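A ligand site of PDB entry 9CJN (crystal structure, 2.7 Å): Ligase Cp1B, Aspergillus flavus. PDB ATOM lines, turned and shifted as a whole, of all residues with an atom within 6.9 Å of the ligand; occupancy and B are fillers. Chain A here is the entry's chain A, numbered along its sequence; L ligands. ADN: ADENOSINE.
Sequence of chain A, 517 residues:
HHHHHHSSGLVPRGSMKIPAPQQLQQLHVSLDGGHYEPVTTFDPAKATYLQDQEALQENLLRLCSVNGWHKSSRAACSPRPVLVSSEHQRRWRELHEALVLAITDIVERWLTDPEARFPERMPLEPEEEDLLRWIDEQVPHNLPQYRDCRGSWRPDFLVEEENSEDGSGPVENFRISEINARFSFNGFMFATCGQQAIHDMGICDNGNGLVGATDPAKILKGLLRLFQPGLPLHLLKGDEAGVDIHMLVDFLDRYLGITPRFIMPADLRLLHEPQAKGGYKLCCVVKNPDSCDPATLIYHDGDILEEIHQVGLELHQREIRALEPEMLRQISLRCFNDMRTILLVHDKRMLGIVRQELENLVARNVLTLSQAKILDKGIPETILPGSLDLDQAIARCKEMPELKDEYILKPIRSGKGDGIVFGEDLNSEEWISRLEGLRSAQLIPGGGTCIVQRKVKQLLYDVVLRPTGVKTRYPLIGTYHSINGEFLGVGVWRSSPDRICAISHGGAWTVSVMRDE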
ATOM      1  N   ASP A 156     -32.042 -12.612  22.110  1.00  0.00           N
ATOM      2  CA  ASP A 156     -32.496 -11.298  22.529  1.00  0.00           C
ATOM      3  C   ASP A 156     -31.335 -10.313  22.430  1.00  0.00           C
ATOM      4  O   ASP A 156     -30.200 -10.630  22.794  1.00  0.00           O
ATOM      5  CB  ASP A 156     -33.007 -11.302  23.975  1.00  0.00           C
ATOM      6  CG  ASP A 156     -34.291 -12.089  24.157  1.00  0.00           C
ATOM      7  OD1 ASP A 156     -35.076 -12.253  23.196  1.00  0.00           O
ATOM      8  OD2 ASP A 156     -34.518 -12.535  25.295  1.00  0.00           O
ATOM      9  N   PHE A 157     -31.599  -9.089  21.982  1.00  0.00           N
ATOM     10  CA  PHE A 157     -30.515  -8.135  21.938  1.00  0.00           C
ATOM     11  C   PHE A 157     -30.975  -6.790  22.478  1.00  0.00           C
ATOM     12  O   PHE A 157     -32.162  -6.435  22.386  1.00  0.00           O
ATOM     13  CB  PHE A 157     -29.951  -7.992  20.512  1.00  0.00           C
ATOM     14  CG  PHE A 157     -30.960  -7.569  19.496  1.00  0.00           C
ATOM     15  CD1 PHE A 157     -31.298  -6.232  19.346  1.00  0.00           C
ATOM     16  CD2 PHE A 157     -31.597  -8.503  18.702  1.00  0.00           C
ATOM     17  CE1 PHE A 157     -32.240  -5.843  18.423  1.00  0.00           C
ATOM     18  CE2 PHE A 157     -32.533  -8.120  17.769  1.00  0.00           C
ATOM     19  CZ  PHE A 157     -32.869  -6.795  17.626  1.00  0.00           C
ATOM     20  N   LEU A 158     -30.031  -6.063  23.056  1.00  0.00           N
ATOM     21  CA  LEU A 158     -30.189  -4.675  23.439  1.00  0.00           C
ATOM     22  C   LEU A 158     -29.508  -3.779  22.405  1.00  0.00           C
ATOM     23  O   LEU A 158     -28.718  -4.223  21.574  1.00  0.00           O
ATOM     24  CB  LEU A 158     -29.580  -4.464  24.823  1.00  0.00           C
ATOM     25  CG  LEU A 158     -29.865  -5.604  25.799  1.00  0.00           C
ATOM     26  CD1 LEU A 158     -28.870  -5.602  26.915  1.00  0.00           C
ATOM     27  CD2 LEU A 158     -31.259  -5.452  26.346  1.00  0.00           C
ATOM     28  N   ARG A 175     -26.283  -5.888  20.895  1.00  0.00           N
ATOM     29  CA  ARG A 175     -25.590  -6.838  21.755  1.00  0.00           C
ATOM     30  C   ARG A 175     -26.573  -7.928  22.163  1.00  0.00           C
ATOM     31  O   ARG A 175     -27.605  -7.638  22.761  1.00  0.00           O
ATOM     32  CB  ARG A 175     -25.055  -6.140  23.007  1.00  0.00           C
ATOM     33  CG  ARG A 175     -23.997  -5.101  22.741  1.00  0.00           C
ATOM     34  CD  ARG A 175     -22.619  -5.663  22.954  1.00  0.00           C
ATOM     35  NE  ARG A 175     -21.592  -4.681  22.629  1.00  0.00           N
ATOM     36  CZ  ARG A 175     -20.307  -4.950  22.475  1.00  0.00           C
ATOM     37  NH1 ARG A 175     -19.845  -6.181  22.625  1.00  0.00           N
ATOM     38  NH2 ARG A 175     -19.471  -3.978  22.143  1.00  0.00           N
ATOM     39  N   ILE A 176     -26.239  -9.178  21.837  1.00  0.00           N
ATOM     40  CA  ILE A 176     -27.051 -10.319  22.245  1.00  0.00           C
ATOM     41  C   ILE A 176     -26.891 -10.553  23.744  1.00  0.00           C
ATOM     42  O   ILE A 176     -25.779 -10.739  24.240  1.00  0.00           O
ATOM     43  CB  ILE A 176     -26.647 -11.575  21.460  1.00  0.00           C
ATOM     44  CG1 ILE A 176     -27.056 -11.447  19.986  1.00  0.00           C
ATOM     45  CG2 ILE A 176     -27.227 -12.808  22.105  1.00  0.00           C
ATOM     46  CD1 ILE A 176     -26.310 -12.398  19.069  1.00  0.00           C
ATOM     47  N   SER A 177     -28.006 -10.529  24.474  1.00  0.00           N
ATOM     48  CA  SER A 177     -27.921 -10.760  25.912  1.00  0.00           C
ATOM     49  C   SER A 177     -28.153 -12.216  26.281  1.00  0.00           C
ATOM     50  O   SER A 177     -27.641 -12.659  27.320  1.00  0.00           O
ATOM     51  CB  SER A 177     -28.922  -9.870  26.657  1.00  0.00           C
ATOM     52  OG  SER A 177     -30.237 -10.019  26.158  1.00  0.00           O
ATOM     53  N   GLU A 178     -28.866 -12.978  25.456  1.00  0.00           N
ATOM     54  CA  GLU A 178     -29.197 -14.365  25.766  1.00  0.00           C
ATOM     55  C   GLU A 178     -29.777 -15.006  24.521  1.00  0.00           C
ATOM     56  O   GLU A 178     -30.395 -14.337  23.687  1.00  0.00           O
ATOM     57  CB  GLU A 178     -30.207 -14.463  26.915  1.00  0.00           C
ATOM     58  CG  GLU A 178     -31.456 -13.629  26.701  1.00  0.00           C
ATOM     59  CD  GLU A 178     -32.077 -13.124  27.994  1.00  0.00           C
ATOM     60  OE1 GLU A 178     -31.325 -12.823  28.973  1.00  0.00           O
ATOM     61  OE2 GLU A 178     -33.318 -13.023  28.031  1.00  0.00           O
ATOM     62  N   PRO A 380     -21.794  -8.919  24.545  1.00  0.00           N
ATOM     63  CA  PRO A 380     -21.119  -8.111  25.573  1.00  0.00           C
ATOM     64  C   PRO A 380     -20.016  -8.916  26.251  1.00  0.00           C
ATOM     65  O   PRO A 380     -20.045 -10.143  26.307  1.00  0.00           O
ATOM     66  CB  PRO A 380     -22.253  -7.769  26.552  1.00  0.00           C
ATOM     67  CG  PRO A 380     -23.266  -8.836  26.361  1.00  0.00           C
ATOM     68  CD  PRO A 380     -23.172  -9.264  24.914  1.00  0.00           C
ATOM     69  N   GLU A 381     -19.012  -8.182  26.745  1.00  0.00           N
ATOM     70  CA  GLU A 381     -17.956  -8.789  27.558  1.00  0.00           C
ATOM     71  C   GLU A 381     -18.570  -9.619  28.678  1.00  0.00           C
ATOM     72  O   GLU A 381     -19.362  -9.126  29.479  1.00  0.00           O
ATOM     73  CB  GLU A 381     -17.057  -7.694  28.124  1.00  0.00           C
ATOM     74  CG  GLU A 381     -15.937  -8.205  29.030  1.00  0.00           C
ATOM     75  CD  GLU A 381     -15.198  -7.063  29.752  1.00  0.00           C
ATOM     76  OE1 GLU A 381     -15.340  -5.875  29.353  1.00  0.00           O
ATOM     77  OE2 GLU A 381     -14.478  -7.356  30.730  1.00  0.00           O
ATOM     78  N   ILE A 408     -22.521  -6.200  35.722  1.00  0.00           N
ATOM     79  CA  ILE A 408     -23.693  -6.795  36.359  1.00  0.00           C
ATOM     80  C   ILE A 408     -23.428  -8.275  36.590  1.00  0.00           C
ATOM     81  O   ILE A 408     -22.464  -8.851  36.081  1.00  0.00           O
ATOM     82  CB  ILE A 408     -24.994  -6.617  35.546  1.00  0.00           C
ATOM     83  CG1 ILE A 408     -24.982  -7.563  34.348  1.00  0.00           C
ATOM     84  CG2 ILE A 408     -25.162  -5.176  35.090  1.00  0.00           C
ATOM     85  CD1 ILE A 408     -26.171  -7.382  33.416  1.00  0.00           C
ATOM     86  N   LYS A 410     -25.490 -11.676  36.160  1.00  0.00           N
ATOM     87  CA  LYS A 410     -26.661 -12.404  35.677  1.00  0.00           C
ATOM     88  C   LYS A 410     -26.621 -13.850  36.177  1.00  0.00           C
ATOM     89  O   LYS A 410     -25.550 -14.469  36.201  1.00  0.00           O
ATOM     90  CB  LYS A 410     -26.718 -12.409  34.155  1.00  0.00           C
ATOM     91  CG  LYS A 410     -27.019 -11.049  33.549  1.00  0.00           C
ATOM     92  CD  LYS A 410     -26.763 -11.030  32.053  1.00  0.00           C
ATOM     93  CE  LYS A 410     -27.873 -11.722  31.276  1.00  0.00           C
ATOM     94  NZ  LYS A 410     -27.616 -11.664  29.810  1.00  0.00           N
ATOM     95  N   ILE A 420     -31.276 -10.161  37.844  1.00  0.00           N
ATOM     96  CA  ILE A 420     -29.979  -9.559  37.568  1.00  0.00           C
ATOM     97  C   ILE A 420     -29.568  -8.641  38.722  1.00  0.00           C
ATOM     98  O   ILE A 420     -30.410  -8.075  39.430  1.00  0.00           O
ATOM     99  CB  ILE A 420     -30.040  -8.800  36.228  1.00  0.00           C
ATOM    100  CG1 ILE A 420     -30.445  -9.738  35.080  1.00  0.00           C
ATOM    101  CG2 ILE A 420     -28.733  -8.108  35.901  1.00  0.00           C
ATOM    102  CD1 ILE A 420     -31.950  -9.879  34.838  1.00  0.00           C
ATOM    103  N   PHE A 422     -26.930  -5.463  39.671  1.00  0.00           N
ATOM    104  CA  PHE A 422     -26.050  -4.402  39.190  1.00  0.00           C
ATOM    105  C   PHE A 422     -25.007  -4.017  40.238  1.00  0.00           C
ATOM    106  O   PHE A 422     -25.288  -3.936  41.433  1.00  0.00           O
ATOM    107  CB  PHE A 422     -26.867  -3.163  38.808  1.00  0.00           C
ATOM    108  CG  PHE A 422     -27.694  -3.335  37.560  1.00  0.00           C
ATOM    109  CD1 PHE A 422     -28.855  -4.096  37.578  1.00  0.00           C
ATOM    110  CD2 PHE A 422     -27.321  -2.721  36.367  1.00  0.00           C
ATOM    111  CE1 PHE A 422     -29.623  -4.253  36.435  1.00  0.00           C
ATOM    112  CE2 PHE A 422     -28.081  -2.874  35.225  1.00  0.00           C
ATOM    113  CZ  PHE A 422     -29.242  -3.638  35.253  1.00  0.00           C
ATOM    114  N   GLN A 453     -21.222  -9.789  33.523  1.00  0.00           N
ATOM    115  CA  GLN A 453     -21.344  -9.179  32.212  1.00  0.00           C
ATOM    116  C   GLN A 453     -21.180  -7.676  32.323  1.00  0.00           C
ATOM    117  O   GLN A 453     -21.581  -7.060  33.319  1.00  0.00           O
ATOM    118  CB  GLN A 453     -22.670  -9.516  31.584  1.00  0.00           C
ATOM    119  CG  GLN A 453     -22.530 -10.010  30.179  1.00  0.00           C
ATOM    120  CD  GLN A 453     -23.857 -10.382  29.563  1.00  0.00           C
ATOM    121  OE1 GLN A 453     -24.911  -9.891  29.977  1.00  0.00           O
ATOM    122  NE2 GLN A 453     -23.815 -11.266  28.570  1.00  0.00           N
ATOM    123  N   ARG A 454     -20.600  -7.075  31.299  1.00  0.00           N
ATOM    124  CA  ARG A 454     -20.533  -5.623  31.239  1.00  0.00           C
ATOM    125  C   ARG A 454     -21.933  -5.058  31.024  1.00  0.00           C
ATOM    126  O   ARG A 454     -22.739  -5.607  30.259  1.00  0.00           O
ATOM    127  CB  ARG A 454     -19.589  -5.166  30.135  1.00  0.00           C
ATOM    128  CG  ARG A 454     -19.678  -3.678  29.836  1.00  0.00           C
ATOM    129  CD  ARG A 454     -18.428  -3.190  29.122  1.00  0.00           C
ATOM    130  NE  ARG A 454     -17.350  -2.925  30.063  1.00  0.00           N
ATOM    131  CZ  ARG A 454     -17.031  -1.730  30.524  1.00  0.00           C
ATOM    132  NH1 ARG A 454     -17.655  -0.633  30.093  1.00  0.00           N
ATOM    133  NH2 ARG A 454     -16.065  -1.612  31.426  1.00  0.00           N
ATOM    134  N   LYS A 455     -22.237  -3.964  31.722  1.00  0.00           N
ATOM    135  CA  LYS A 455     -23.527  -3.303  31.586  1.00  0.00           C
ATOM    136  C   LYS A 455     -23.588  -2.596  30.233  1.00  0.00           C
ATOM    137  O   LYS A 455     -22.728  -1.761  29.924  1.00  0.00           O
ATOM    138  CB  LYS A 455     -23.746  -2.323  32.734  1.00  0.00           C
ATOM    139  CG  LYS A 455     -25.059  -1.535  32.687  1.00  0.00           C
ATOM    140  CD  LYS A 455     -25.169  -0.585  33.884  1.00  0.00           C
ATOM    141  CE  LYS A 455     -25.972   0.671  33.560  1.00  0.00           C
ATOM    142  NZ  LYS A 455     -27.444   0.506  33.752  1.00  0.00           N
ATOM    143  N   VAL A 456     -24.577  -2.948  29.429  1.00  0.00           N
ATOM    144  CA  VAL A 456     -24.844  -2.246  28.183  1.00  0.00           C
ATOM    145  C   VAL A 456     -25.566  -0.945  28.502  1.00  0.00           C
ATOM    146  O   VAL A 456     -26.558  -0.941  29.253  1.00  0.00           O
ATOM    147  CB  VAL A 456     -25.671  -3.130  27.231  1.00  0.00           C
ATOM    148  CG1 VAL A 456     -26.063  -2.344  25.968  1.00  0.00           C
ATOM    149  CG2 VAL A 456     -24.913  -4.405  26.850  1.00  0.00           C
ATOM    150  N   LYS A 457     -25.051   0.162  27.973  1.00  0.00           N
ATOM    151  CA  LYS A 457     -25.667   1.483  28.125  1.00  0.00           C
ATOM    152  C   LYS A 457     -26.668   1.658  26.988  1.00  0.00           C
ATOM    153  O   LYS A 457     -26.318   2.051  25.874  1.00  0.00           O
ATOM    154  CB  LYS A 457     -24.596   2.567  28.120  1.00  0.00           C
ATOM    155  CG  LYS A 457     -25.090   3.998  28.179  1.00  0.00           C
ATOM    156  CD  LYS A 457     -25.374   4.451  29.607  1.00  0.00           C
ATOM    157  CE  LYS A 457     -25.482   5.968  29.696  1.00  0.00           C
ATOM    158  NZ  LYS A 457     -26.354   6.523  28.625  1.00  0.00           N
ATOM    159  N   GLN A 458     -27.935   1.332  27.262  1.00  0.00           N
ATOM    160  CA  GLN A 458     -28.948   1.275  26.224  1.00  0.00           C
ATOM    161  C   GLN A 458     -29.384   2.671  25.774  1.00  0.00           C
ATOM    162  O   GLN A 458     -29.457   3.611  26.569  1.00  0.00           O
ATOM    163  CB  GLN A 458     -30.160   0.495  26.708  1.00  0.00           C
ATOM    164  CG  GLN A 458     -29.815  -0.913  27.142  1.00  0.00           C
ATOM    165  CD  GLN A 458     -30.999  -1.663  27.699  1.00  0.00           C
ATOM    166  OE1 GLN A 458     -31.787  -2.240  26.950  1.00  0.00           O
ATOM    167  NE2 GLN A 458     -31.137  -1.655  29.010  1.00  0.00           N
ATOM    168  N   PRO A 475     -36.032   2.167  26.584  1.00  0.00           N
ATOM    169  CA  PRO A 475     -35.213   1.364  25.681  1.00  0.00           C
ATOM    170  C   PRO A 475     -36.041   0.333  24.932  1.00  0.00           C
ATOM    171  O   PRO A 475     -37.192   0.044  25.261  1.00  0.00           O
ATOM    172  CB  PRO A 475     -34.200   0.684  26.615  1.00  0.00           C
ATOM    173  CG  PRO A 475     -34.877   0.647  27.927  1.00  0.00           C
ATOM    174  CD  PRO A 475     -35.718   1.891  27.999  1.00  0.00           C
ATOM    175  N   LEU A 476     -35.442  -0.191  23.870  1.00  0.00           N
ATOM    176  CA  LEU A 476     -36.062  -1.195  23.020  1.00  0.00           C
ATOM    177  C   LEU A 476     -35.300  -2.502  23.172  1.00  0.00           C
ATOM    178  O   LEU A 476     -34.073  -2.518  23.059  1.00  0.00           O
ATOM    179  CB  LEU A 476     -36.059  -0.768  21.547  1.00  0.00           C
ATOM    180  CG  LEU A 476     -37.032   0.344  21.146  1.00  0.00           C
ATOM    181  CD1 LEU A 476     -36.606   0.862  19.822  1.00  0.00           C
ATOM    182  CD2 LEU A 476     -38.428  -0.187  21.063  1.00  0.00           C
ATOM    183  N   ILE A 477     -36.026  -3.577  23.421  1.00  0.00           N
ATOM    184  CA  ILE A 477     -35.471  -4.916  23.527  1.00  0.00           C
ATOM    185  C   ILE A 477     -35.900  -5.672  22.285  1.00  0.00           C
ATOM    186  O   ILE A 477     -37.096  -5.800  22.003  1.00  0.00           O
ATOM    187  CB  ILE A 477     -35.949  -5.641  24.793  1.00  0.00           C
ATOM    188  CG1 ILE A 477     -35.384  -4.977  26.063  1.00  0.00           C
ATOM    189  CG2 ILE A 477     -35.535  -7.095  24.740  1.00  0.00           C
ATOM    190  CD1 ILE A 477     -36.029  -3.657  26.448  1.00  0.00           C
ATOM    191  N   ARG A 494     -40.027  -5.180  22.378  1.00  0.00           N
ATOM    192  CA  ARG A 494     -40.577  -5.037  23.708  1.00  0.00           C
ATOM    193  C   ARG A 494     -39.947  -3.812  24.342  1.00  0.00           C
ATOM    194  O   ARG A 494     -38.868  -3.376  23.945  1.00  0.00           O
ATOM    195  CB  ARG A 494     -40.318  -6.283  24.564  1.00  0.00           C
ATOM    196  CG  ARG A 494     -41.202  -7.488  24.212  1.00  0.00           C
ATOM    197  CD  ARG A 494     -40.682  -8.772  24.834  1.00  0.00           C
ATOM    198  NE  ARG A 494     -39.410  -9.184  24.239  1.00  0.00           N
ATOM    199  CZ  ARG A 494     -38.576 -10.043  24.797  1.00  0.00           C
ATOM    200  NH1 ARG A 494     -38.832 -10.605  25.966  1.00  0.00           N
ATOM    201  NH2 ARG A 494     -37.443 -10.352  24.167  1.00  0.00           N
HETATM  202  O5' ADN L   1     -32.850  -9.677  29.275  1.00  0.00           O
HETATM  203  C5' ADN L   1     -33.150  -8.337  28.892  1.00  0.00           C
HETATM  204  C4' ADN L   1     -32.927  -7.373  30.032  1.00  0.00           C
HETATM  205  O4' ADN L   1     -31.901  -7.886  30.926  1.00  0.00           O
HETATM  206  C3' ADN L   1     -32.423  -5.987  29.631  1.00  0.00           C
HETATM  207  O3' ADN L   1     -33.453  -5.105  29.229  1.00  0.00           O
HETATM  208  C2' ADN L   1     -31.682  -5.520  30.876  1.00  0.00           C
HETATM  209  O2' ADN L   1     -32.591  -5.054  31.863  1.00  0.00           O
HETATM  210  C1' ADN L   1     -31.071  -6.833  31.379  1.00  0.00           C
HETATM  211  N9  ADN L   1     -29.699  -7.067  30.872  1.00  0.00           N
HETATM  212  C8  ADN L   1     -29.223  -8.282  30.437  1.00  0.00           C
HETATM  213  N7  ADN L   1     -27.979  -8.241  30.050  1.00  0.00           N
HETATM  214  C5  ADN L   1     -27.597  -6.938  30.246  1.00  0.00           C
HETATM  215  C6  ADN L   1     -26.381  -6.270  30.026  1.00  0.00           C
HETATM  216  N6  ADN L   1     -25.289  -6.873  29.528  1.00  0.00           N
HETATM  217  N1  ADN L   1     -26.330  -4.957  30.325  1.00  0.00           N
HETATM  218  C2  ADN L   1     -27.410  -4.347  30.806  1.00  0.00           C
HETATM  219  N3  ADN L   1     -28.598  -4.878  31.062  1.00  0.00           N
HETATM  220  C4  ADN L   1     -28.652  -6.182  30.764  1.00  0.00           C
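N of Val 456 is in hydrogen-bond range of N1 of the ligand, at 2.8 Å. A nitrogen (N6) of the ligand is in hydrogen-bond range of the backbone carbonyl oxygen (O) of Arg 454 (2.9 Å). A nitrogen (N6) of the ligand sits at hydrogen-bond distance from the side-chain amide oxygen (OE1) of Gln 453, 3.1 Å away. The side-chain amino group (NZ) of Lys 410 lies within hydrogen-bond range of a nitrogen (N7) of the ligand (3.5 Å).
The guanidinium group (NE) of Arg 454 lies within salt-bridge range of the side-chain carboxylate (OE1) of Glu 381, 3.6 Å away. The side-chain amide oxygen (OE1) of Gln 453 sits close to the side-chain amino group (NZ) of Lys 410 (3.2 Å). NZ of Lys 410 is in salt-bridge range of OE1 of Glu 178 (3.97 Å). The backbone carbonyl oxygen (O) of Ser 177 lies within hydrogen-bond range of the side-chain amino group (NZ) of Lys 410. N of Asp 156 is in hydrogen-bond range of O of Glu 178, 2.9 Å away. The backbone NH of Leu 158 is in hydrogen-bond range of the backbone carbonyl oxygen of Arg 175 (2.9 Å). The backbone carbonyl oxygen of Arg 494 is in hydrogen-bond range of the backbone NH of Ile 477 (2.9 Å). The backbone NH (N) of Ser 177 sits at hydrogen-bond distance from the backbone carbonyl oxygen (O) of Asp 156 (2.8 Å).
CD2 of Leu 158 touches C3' of the ligand, at 3.5 Å. Ser 177 touches the ligand (CB to N7, 3.9 Å). OE1 of Glu 178 touches O5' of the ligand, 3.5 Å away. Ile 408 touches the ligand (CD1 to C5, 3.5 Å). Lys 455 touches the ligand. Ile 477 touches the ligand. Of the 23 residues printed, 10 come within 4 Å of the ligand. Along chain A the residues within 4 Å of the ligand span positions 158 to 477. The nearest printed residue that does not touch the ligand is Gln 458 (4.02 Å).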
